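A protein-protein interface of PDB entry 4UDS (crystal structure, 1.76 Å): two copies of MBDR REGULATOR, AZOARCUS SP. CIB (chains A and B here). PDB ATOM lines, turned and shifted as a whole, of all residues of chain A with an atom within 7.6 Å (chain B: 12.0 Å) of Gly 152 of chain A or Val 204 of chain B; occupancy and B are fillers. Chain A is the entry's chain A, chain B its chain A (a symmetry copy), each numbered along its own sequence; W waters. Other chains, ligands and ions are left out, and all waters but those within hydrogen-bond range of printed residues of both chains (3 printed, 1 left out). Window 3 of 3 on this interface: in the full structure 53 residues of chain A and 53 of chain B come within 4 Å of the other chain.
Water W1 bridges OD1 of Asn 200 of chain A and NH2 of Arg 155 of chain B. Water W3 bridges the side-chain amide oxygen of Asn 200 of chain B and the guanidinium group of Arg 155 of chain A. Water W2 bridges O of Asn 200 of chain A (3.1 Å) and NH2 of Arg 155 of chain B (3.2 Å).
Hydrophobic or aromatic side chains of chain A within 4 Å of the printed part of chain B: Val 153, Phe 154 and Leu 199. Printed residues of chain B that touch a printed residue of chain A: Arg 155, Ser 196, Asn 200, Gly 201, Leu 202, Ile 203 and Val 204. Hydrophobic or aromatic side chains of chain B that line the printed part of chain A: Leu 202, Ile 203 and Val 204. Among the printed residues, 18 pairs touch across the chains. Among the printed residues, no Asp or Glu carboxylate lies within 4 Å of a Lys or Arg side-chain nitrogen of the other chain.
Arg 155 of chain A touches Asn 200 of chain B, and with the chains exchanged Asn 200 of chain A touches Arg 155 of chain B. Asn 200 of chain A touches its own counterpart, Asn 200 of chain B. Positions printed for both chains: 155, 199 and 200.
Among the printed residues, merely in contact across the chains: Gly 152 of chain A with Val 204 of chain B, Val 153 of chain A with Ile 203 of chain B, Phe 154 of chain A with Leu 202 of chain B, Phe 154 of chain A with Ile 203 of chain B, Phe 154 of chain A with Val 204 of chain B, Arg 155 of chain A with Asn 200 of chain B, Arg 155 of chain A with Val 204 of chain B, Leu 199 of chain A with Gly 201 of chain B, Asn 200 of chain A with Arg 155 of chain B, Asn 200 of chain A with Gly 201 of chain B and Asn 200 of chain A with Ile 203 of chain B.
Gly 152 of chain A touches just one residue of chain B: Val 204. Of chain A, only Gly 152, Val 153, Phe 154 and Arg 155 come within 4 Å of Val 204 of chain B. No residue of chain B comes within 4 Å of Gly 148 of chain A. No residue of chain B comes within 4 Å of Thr 150 of chain A. Printed residues of chain B within 4 Å of Asn 200 of chain A: Arg 155 (3.3 Å), Asn 200 (3.4 Å), Gly 201 (3.7 Å) and Ile 203 (3.8 Å). Of the printed residues of chain B, Arg 155 of chain A touches Ser 196, Asn 200, Gly 201, Leu 202 and Val 204. Of the printed residues of chain A, Leu 202 of chain B touches Phe 154, Arg 155 and Leu 199. Printed residues of chain A within 4 Å of Arg 155 of chain B: Asn 200 (3.3 Å). Printed residues of chain B within 4 Å of Phe 154 of chain A: Leu 202 (3.1 Å), Ile 203 (3.7 Å) and Val 204 (3.5 Å). Gln 149 of chain A touches none of the printed residues of chain B. Val 197 of chain B touches none of the printed residues of chain A. The nearest residue of chain B that does not touch Gly 152 of chain A is Ile 203 of chain B (6.5 Å). The nearest residue of chain A that does not touch Val 204 of chain B is Ser 156 of chain A (5.4 Å).
The backbone carbonyl oxygen of Gly 148 of chain A lies within hydrogen-bond range of the backbone NH of Val 153 of chain A (3.0 Å). N of Phe 154 of chain A sits at hydrogen-bond distance from O of Gly 148 of chain A, 3.2 Å away. O of Arg 155 of chain A sits at hydrogen-bond distance from NE2 of Gln 149 of chain A, at 3.0 Å. The backbone carbonyl oxygen (O) of Ser 196 of chain B is in hydrogen-bond range of the backbone NH (N) of Gly 201 of chain B, 3.4 Å away.
The backbone carbonyl oxygen (O) of Leu 199 of chain A lies within hydrogen-bond range of the backbone NH (N) of Leu 202 of chain B, 3.1 Å away. The backbone carbonyl oxygen (O) of Val 153 of chain A lies within hydrogen-bond range of the backbone NH (N) of Val 204 of chain B, 3.0 Å away. The backbone carbonyl oxygen (O) of Gly 201 of chain B is in hydrogen-bond range of the guanidinium group (NH2) of Arg 155 of chain A, 3.0 Å away. The backbone NH of Arg 155 of chain A is in hydrogen-bond range of the backbone carbonyl oxygen of Leu 202 of chain B (2.8 Å). The backbone carbonyl oxygen (O) of Leu 199 of chain A is in hydrogen-bond range of the backbone NH (N) of Ile 203 of chain B, at 3.0 Å. The guanidinium group of Arg 155 of chain A lies within hydrogen-bond range of the backbone carbonyl oxygen of Ser 196 of chain B. O of Asn 200 of chain A sits close to O of Asn 200 of chain B, 3.4 Å away.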
ATOM      1  N   LEU A  86      -5.295  38.116  14.643  1.00  0.00           N
ATOM      2  CA  LEU A  86      -4.339  37.053  14.319  1.00  0.00           C
ATOM      3  C   LEU A  86      -4.960  35.650  14.235  1.00  0.00           C
ATOM      4  O   LEU A  86      -6.074  35.456  14.574  1.00  0.00           O
ATOM      5  CB  LEU A  86      -3.202  36.994  15.310  1.00  0.00           C
ATOM      6  CG  LEU A  86      -2.522  38.339  15.577  1.00  0.00           C
ATOM      7  CD1 LEU A  86      -1.604  38.281  16.758  1.00  0.00           C
ATOM      8  CD2 LEU A  86      -1.806  38.851  14.364  1.00  0.00           C
ATOM      9  N   ALA A 146      -1.173  27.561   8.581  1.00  0.00           N
ATOM     10  CA  ALA A 146      -0.043  28.094   7.873  1.00  0.00           C
ATOM     11  C   ALA A 146       0.100  29.590   8.113  1.00  0.00           C
ATOM     12  O   ALA A 146       1.167  30.070   8.284  1.00  0.00           O
ATOM     13  CB  ALA A 146      -0.197  27.841   6.404  1.00  0.00           C
ATOM     14  N   GLN A 147      -1.015  30.298   8.151  1.00  0.00           N
ATOM     15  CA  GLN A 147      -0.978  31.739   8.398  1.00  0.00           C
ATOM     16  C   GLN A 147      -0.423  32.037   9.760  1.00  0.00           C
ATOM     17  O   GLN A 147       0.381  32.860   9.921  1.00  0.00           O
ATOM     18  CB  GLN A 147      -2.356  32.321   8.250  1.00  0.00           C
ATOM     19  CG  GLN A 147      -2.483  33.832   8.267  1.00  0.00           C
ATOM     20  CD  GLN A 147      -1.366  34.571   7.569  1.00  0.00           C
ATOM     21  OE1 GLN A 147      -1.028  34.283   6.446  1.00  0.00           O
ATOM     22  NE2 GLN A 147      -0.810  35.560   8.237  1.00  0.00           N
ATOM     23  N   GLY A 148      -0.888  31.300  10.741  1.00  0.00           N
ATOM     24  CA  GLY A 148      -0.429  31.482  12.094  1.00  0.00           C
ATOM     25  C   GLY A 148       1.063  31.201  12.243  1.00  0.00           C
ATOM     26  O   GLY A 148       1.734  31.828  12.987  1.00  0.00           O
ATOM     27  N   GLN A 149       1.544  30.233  11.510  1.00  0.00           N
ATOM     28  CA  GLN A 149       2.952  29.917  11.502  1.00  0.00           C
ATOM     29  C   GLN A 149       3.776  31.080  10.936  1.00  0.00           C
ATOM     30  O   GLN A 149       4.712  31.490  11.502  1.00  0.00           O
ATOM     31  CB  GLN A 149       3.178  28.637  10.731  1.00  0.00           C
ATOM     32  CG  GLN A 149       2.757  27.399  11.508  1.00  0.00           C
ATOM     33  CD  GLN A 149       2.866  26.107  10.715  1.00  0.00           C
ATOM     34  OE1 GLN A 149       2.698  26.130   9.556  1.00  0.00           O
ATOM     35  NE2 GLN A 149       3.125  24.999  11.381  1.00  0.00           N
ATOM     36  N   THR A 150       3.293  31.659   9.856  1.00  0.00           N
ATOM     37  CA  THR A 150       3.898  32.861   9.289  1.00  0.00           C
ATOM     38  C   THR A 150       3.929  34.006  10.288  1.00  0.00           C
ATOM     39  O   THR A 150       4.884  34.668  10.387  1.00  0.00           O
ATOM     40  CB  THR A 150       3.078  33.380   8.079  1.00  0.00           C
ATOM     41  OG1 THR A 150       3.106  32.415   7.065  1.00  0.00           O
ATOM     42  CG2 THR A 150       3.650  34.664   7.527  1.00  0.00           C
ATOM     43  N   GLU A 151       2.851  34.207  11.012  1.00  0.00           N
ATOM     44  CA  GLU A 151       2.742  35.268  11.980  1.00  0.00           C
ATOM     45  C   GLU A 151       3.546  35.041  13.231  1.00  0.00           C
ATOM     46  O   GLU A 151       3.667  35.924  14.002  1.00  0.00           O
ATOM     47  CB  GLU A 151       1.290  35.526  12.361  1.00  0.00           C
ATOM     48  CG  GLU A 151       0.350  35.695  11.186  1.00  0.00           C
ATOM     49  CD  GLU A 151      -1.144  35.831  11.572  1.00  0.00           C
ATOM     50  OE1 GLU A 151      -1.623  35.144  12.451  1.00  0.00           O
ATOM     51  OE2 GLU A 151      -1.847  36.620  10.942  1.00  0.00           O
ATOM     52  N   GLY A 152       3.999  33.825  13.462  1.00  0.00           N
ATOM     53  CA  GLY A 152       4.672  33.506  14.685  1.00  0.00           C
ATOM     54  C   GLY A 152       3.764  33.190  15.859  1.00  0.00           C
ATOM     55  O   GLY A 152       4.207  33.078  16.947  1.00  0.00           O
ATOM     56  N   VAL A 153       2.478  33.133  15.606  1.00  0.00           N
ATOM     57  CA  VAL A 153       1.514  32.653  16.585  1.00  0.00           C
ATOM     58  C   VAL A 153       1.505  31.140  16.894  1.00  0.00           C
ATOM     59  O   VAL A 153       1.369  30.743  18.009  1.00  0.00           O
ATOM     60  CB  VAL A 153       0.101  33.128  16.237  1.00  0.00           C
ATOM     61  CG1 VAL A 153      -0.859  32.695  17.286  1.00  0.00           C
ATOM     62  CG2 VAL A 153       0.084  34.628  16.132  1.00  0.00           C
ATOM     63  N   PHE A 154       1.569  30.339  15.855  1.00  0.00           N
ATOM     64  CA  PHE A 154       1.568  28.899  15.993  1.00  0.00           C
ATOM     65  C   PHE A 154       2.944  28.268  15.790  1.00  0.00           C
ATOM     66  O   PHE A 154       3.720  28.720  15.019  1.00  0.00           O
ATOM     67  CB  PHE A 154       0.647  28.236  14.970  1.00  0.00           C
ATOM     68  CG  PHE A 154      -0.788  28.624  15.066  1.00  0.00           C
ATOM     69  CD1 PHE A 154      -1.350  28.908  16.265  1.00  0.00           C
ATOM     70  CD2 PHE A 154      -1.588  28.627  13.958  1.00  0.00           C
ATOM     71  CE1 PHE A 154      -2.682  29.236  16.375  1.00  0.00           C
ATOM     72  CE2 PHE A 154      -2.915  28.952  14.035  1.00  0.00           C
ATOM     73  CZ  PHE A 154      -3.471  29.247  15.244  1.00  0.00           C
ATOM     74  N   ARG A 155       3.166  27.133  16.437  1.00  0.00           N
ATOM     75  CA  ARG A 155       4.401  26.411  16.328  1.00  0.00           C
ATOM     76  C   ARG A 155       4.698  25.943  14.914  1.00  0.00           C
ATOM     77  O   ARG A 155       3.811  25.729  14.171  1.00  0.00           O
ATOM     78  CB  ARG A 155       4.375  25.187  17.229  1.00  0.00           C
ATOM     79  CG  ARG A 155       3.470  24.114  16.720  1.00  0.00           C
ATOM     80  CD  ARG A 155       3.874  22.781  17.284  1.00  0.00           C
ATOM     81  NE  ARG A 155       3.480  22.584  18.631  1.00  0.00           N
ATOM     82  CZ  ARG A 155       4.119  21.915  19.583  1.00  0.00           C
ATOM     83  NH1 ARG A 155       5.305  21.361  19.465  1.00  0.00           N
ATOM     84  NH2 ARG A 155       3.511  21.816  20.714  1.00  0.00           N
ATOM     85  N   SER A 156       5.992  25.839  14.608  1.00  0.00           N
ATOM     86  CA  SER A 156       6.504  25.476  13.312  1.00  0.00           C
ATOM     87  C   SER A 156       7.384  24.224  13.297  1.00  0.00           C
ATOM     88  O   SER A 156       8.057  23.964  12.372  1.00  0.00           O
ATOM     89  CB  SER A 156       7.222  26.638  12.656  1.00  0.00           C
ATOM     90  OG  SER A 156       8.136  27.213  13.500  1.00  0.00           O
ATOM     91  N   LEU A 199      -5.192  24.982  21.652  1.00  0.00           N
ATOM     92  CA  LEU A 199      -4.351  26.178  21.790  1.00  0.00           C
ATOM     93  C   LEU A 199      -3.076  25.994  22.648  1.00  0.00           C
ATOM     94  O   LEU A 199      -1.971  26.284  22.231  1.00  0.00           O
ATOM     95  CB  LEU A 199      -5.198  27.325  22.371  1.00  0.00           C
ATOM     96  CG  LEU A 199      -6.311  28.066  21.615  1.00  0.00           C
ATOM     97  CD1 LEU A 199      -6.976  29.075  22.503  1.00  0.00           C
ATOM     98  CD2 LEU A 199      -5.781  28.827  20.428  1.00  0.00           C
ATOM     99  N   ASN A 200      -3.265  25.513  23.860  1.00  0.00           N
ATOM    100  CA  ASN A 200      -2.161  25.337  24.772  1.00  0.00           C
ATOM    101  C   ASN A 200      -1.781  23.945  25.305  1.00  0.00           C
ATOM    102  O   ASN A 200      -0.906  23.857  26.085  1.00  0.00           O
ATOM    103  CB  ASN A 200      -2.300  26.311  25.928  1.00  0.00           C
ATOM    104  CG  ASN A 200      -2.296  27.746  25.454  1.00  0.00           C
ATOM    105  OD1 ASN A 200      -3.299  28.331  25.331  1.00  0.00           O
ATOM    106  ND2 ASN A 200      -1.159  28.243  25.096  1.00  0.00           N
ATOM    107  N   ARG B 155      -2.585  20.732  33.281  1.00  0.00           N
ATOM    108  CA  ARG B 155      -3.437  21.822  33.661  1.00  0.00           C
ATOM    109  C   ARG B 155      -4.685  21.377  34.403  1.00  0.00           C
ATOM    110  O   ARG B 155      -5.133  20.308  34.202  1.00  0.00           O
ATOM    111  CB  ARG B 155      -3.878  22.598  32.430  1.00  0.00           C
ATOM    112  CG  ARG B 155      -4.867  21.850  31.599  1.00  0.00           C
ATOM    113  CD  ARG B 155      -5.667  22.804  30.756  1.00  0.00           C
ATOM    114  NE  ARG B 155      -4.968  23.293  29.625  1.00  0.00           N
ATOM    115  CZ  ARG B 155      -5.055  24.493  29.063  1.00  0.00           C
ATOM    116  NH1 ARG B 155      -5.770  25.499  29.514  1.00  0.00           N
ATOM    117  NH2 ARG B 155      -4.368  24.668  27.987  1.00  0.00           N
ATOM    118  N   SER B 196       2.422  16.283  19.961  1.00  0.00           N
ATOM    119  CA  SER B 196       2.835  17.638  20.150  1.00  0.00           C
ATOM    120  C   SER B 196       1.668  18.547  20.594  1.00  0.00           C
ATOM    121  O   SER B 196       1.807  19.348  21.449  1.00  0.00           O
ATOM    122  CB  SER B 196       3.395  18.173  18.836  1.00  0.00           C
ATOM    123  OG  SER B 196       4.614  17.540  18.571  1.00  0.00           O
ATOM    124  N   VAL B 197       0.545  18.395  19.904  1.00  0.00           N
ATOM    125  CA  VAL B 197      -0.625  19.171  20.215  1.00  0.00           C
ATOM    126  C   VAL B 197      -1.231  18.818  21.559  1.00  0.00           C
ATOM    127  O   VAL B 197      -1.509  19.656  22.297  1.00  0.00           O
ATOM    128  CB  VAL B 197      -1.703  19.051  19.129  1.00  0.00           C
ATOM    129  CG1 VAL B 197      -3.016  19.727  19.510  1.00  0.00           C
ATOM    130  CG2 VAL B 197      -1.168  19.653  17.872  1.00  0.00           C
ATOM    131  N   LEU B 199       0.208  17.536  24.133  1.00  0.00           N
ATOM    132  CA  LEU B 199       1.091  17.997  25.214  1.00  0.00           C
ATOM    133  C   LEU B 199       1.223  19.533  25.350  1.00  0.00           C
ATOM    134  O   LEU B 199       1.017  20.106  26.402  1.00  0.00           O
ATOM    135  CB  LEU B 199       2.487  17.377  25.021  1.00  0.00           C
ATOM    136  CG  LEU B 199       2.827  15.894  25.231  1.00  0.00           C
ATOM    137  CD1 LEU B 199       4.262  15.625  24.887  1.00  0.00           C
ATOM    138  CD2 LEU B 199       2.647  15.469  26.665  1.00  0.00           C
ATOM    139  N   ASN B 200       1.581  20.177  24.258  1.00  0.00           N
ATOM    140  CA  ASN B 200       1.781  21.605  24.267  1.00  0.00           C
ATOM    141  C   ASN B 200       0.921  22.537  23.395  1.00  0.00           C
ATOM    142  O   ASN B 200       1.154  23.689  23.398  1.00  0.00           O
ATOM    143  CB  ASN B 200       3.253  21.911  24.052  1.00  0.00           C
ATOM    144  CG  ASN B 200       4.113  21.307  25.138  1.00  0.00           C
ATOM    145  OD1 ASN B 200       4.680  20.304  24.953  1.00  0.00           O
ATOM    146  ND2 ASN B 200       4.101  21.890  26.289  1.00  0.00           N
ATOM    147  N   GLY B 201       0.000  22.012  22.627  1.00  0.00           N
ATOM    148  CA  GLY B 201      -0.884  22.852  21.867  1.00  0.00           C
ATOM    149  C   GLY B 201      -0.271  23.447  20.617  1.00  0.00           C
ATOM    150  O   GLY B 201       0.787  23.109  20.287  1.00  0.00           O
ATOM    151  N   LEU B 202      -0.980  24.373  19.989  1.00  0.00           N
ATOM    152  CA  LEU B 202      -0.531  25.057  18.772  1.00  0.00           C
ATOM    153  C   LEU B 202       0.231  26.373  19.000  1.00  0.00           C
ATOM    154  O   LEU B 202       1.011  26.747  18.206  1.00  0.00           O
ATOM    155  CB  LEU B 202      -1.734  25.383  17.913  1.00  0.00           C
ATOM    156  CG  LEU B 202      -2.497  24.199  17.359  1.00  0.00           C
ATOM    157  CD1 LEU B 202      -3.762  24.677  16.729  1.00  0.00           C
ATOM    158  CD2 LEU B 202      -1.677  23.501  16.306  1.00  0.00           C
ATOM    159  N   ILE B 203      -0.063  27.036  20.089  1.00  0.00           N
ATOM    160  CA  ILE B 203       0.457  28.374  20.364  1.00  0.00           C
ATOM    161  C   ILE B 203       1.905  28.297  20.762  1.00  0.00           C
ATOM    162  O   ILE B 203       2.279  27.445  21.521  1.00  0.00           O
ATOM    163  CB  ILE B 203      -0.376  29.106  21.431  1.00  0.00           C
ATOM    164  CG1 ILE B 203      -1.804  29.174  20.994  1.00  0.00           C
ATOM    165  CG2 ILE B 203       0.136  30.499  21.676  1.00  0.00           C
ATOM    166  CD1 ILE B 203      -2.090  30.160  19.922  1.00  0.00           C
ATOM    167  N   VAL B 204       2.693  29.222  20.235  1.00  0.00           N
ATOM    168  CA  VAL B 204       4.098  29.234  20.469  1.00  0.00           C
ATOM    169  C   VAL B 204       4.427  29.494  21.917  1.00  0.00           C
ATOM    170  O   VAL B 204       3.991  30.453  22.485  1.00  0.00           O
ATOM    171  CB  VAL B 204       4.809  30.267  19.597  1.00  0.00           C
ATOM    172  CG1 VAL B 204       4.973  29.733  18.227  1.00  0.00           C
ATOM    173  CG2 VAL B 204       4.006  31.541  19.544  1.00  0.00           C
HETATM  174  O   HOH W   1      -5.531  27.552  26.931  1.00  0.00           O
HETATM  175  O   HOH W   2      -1.522  23.713  29.083  1.00  0.00           O
HETATM  176  O   HOH W   3       5.386  19.615  22.274  1.00  0.00           O
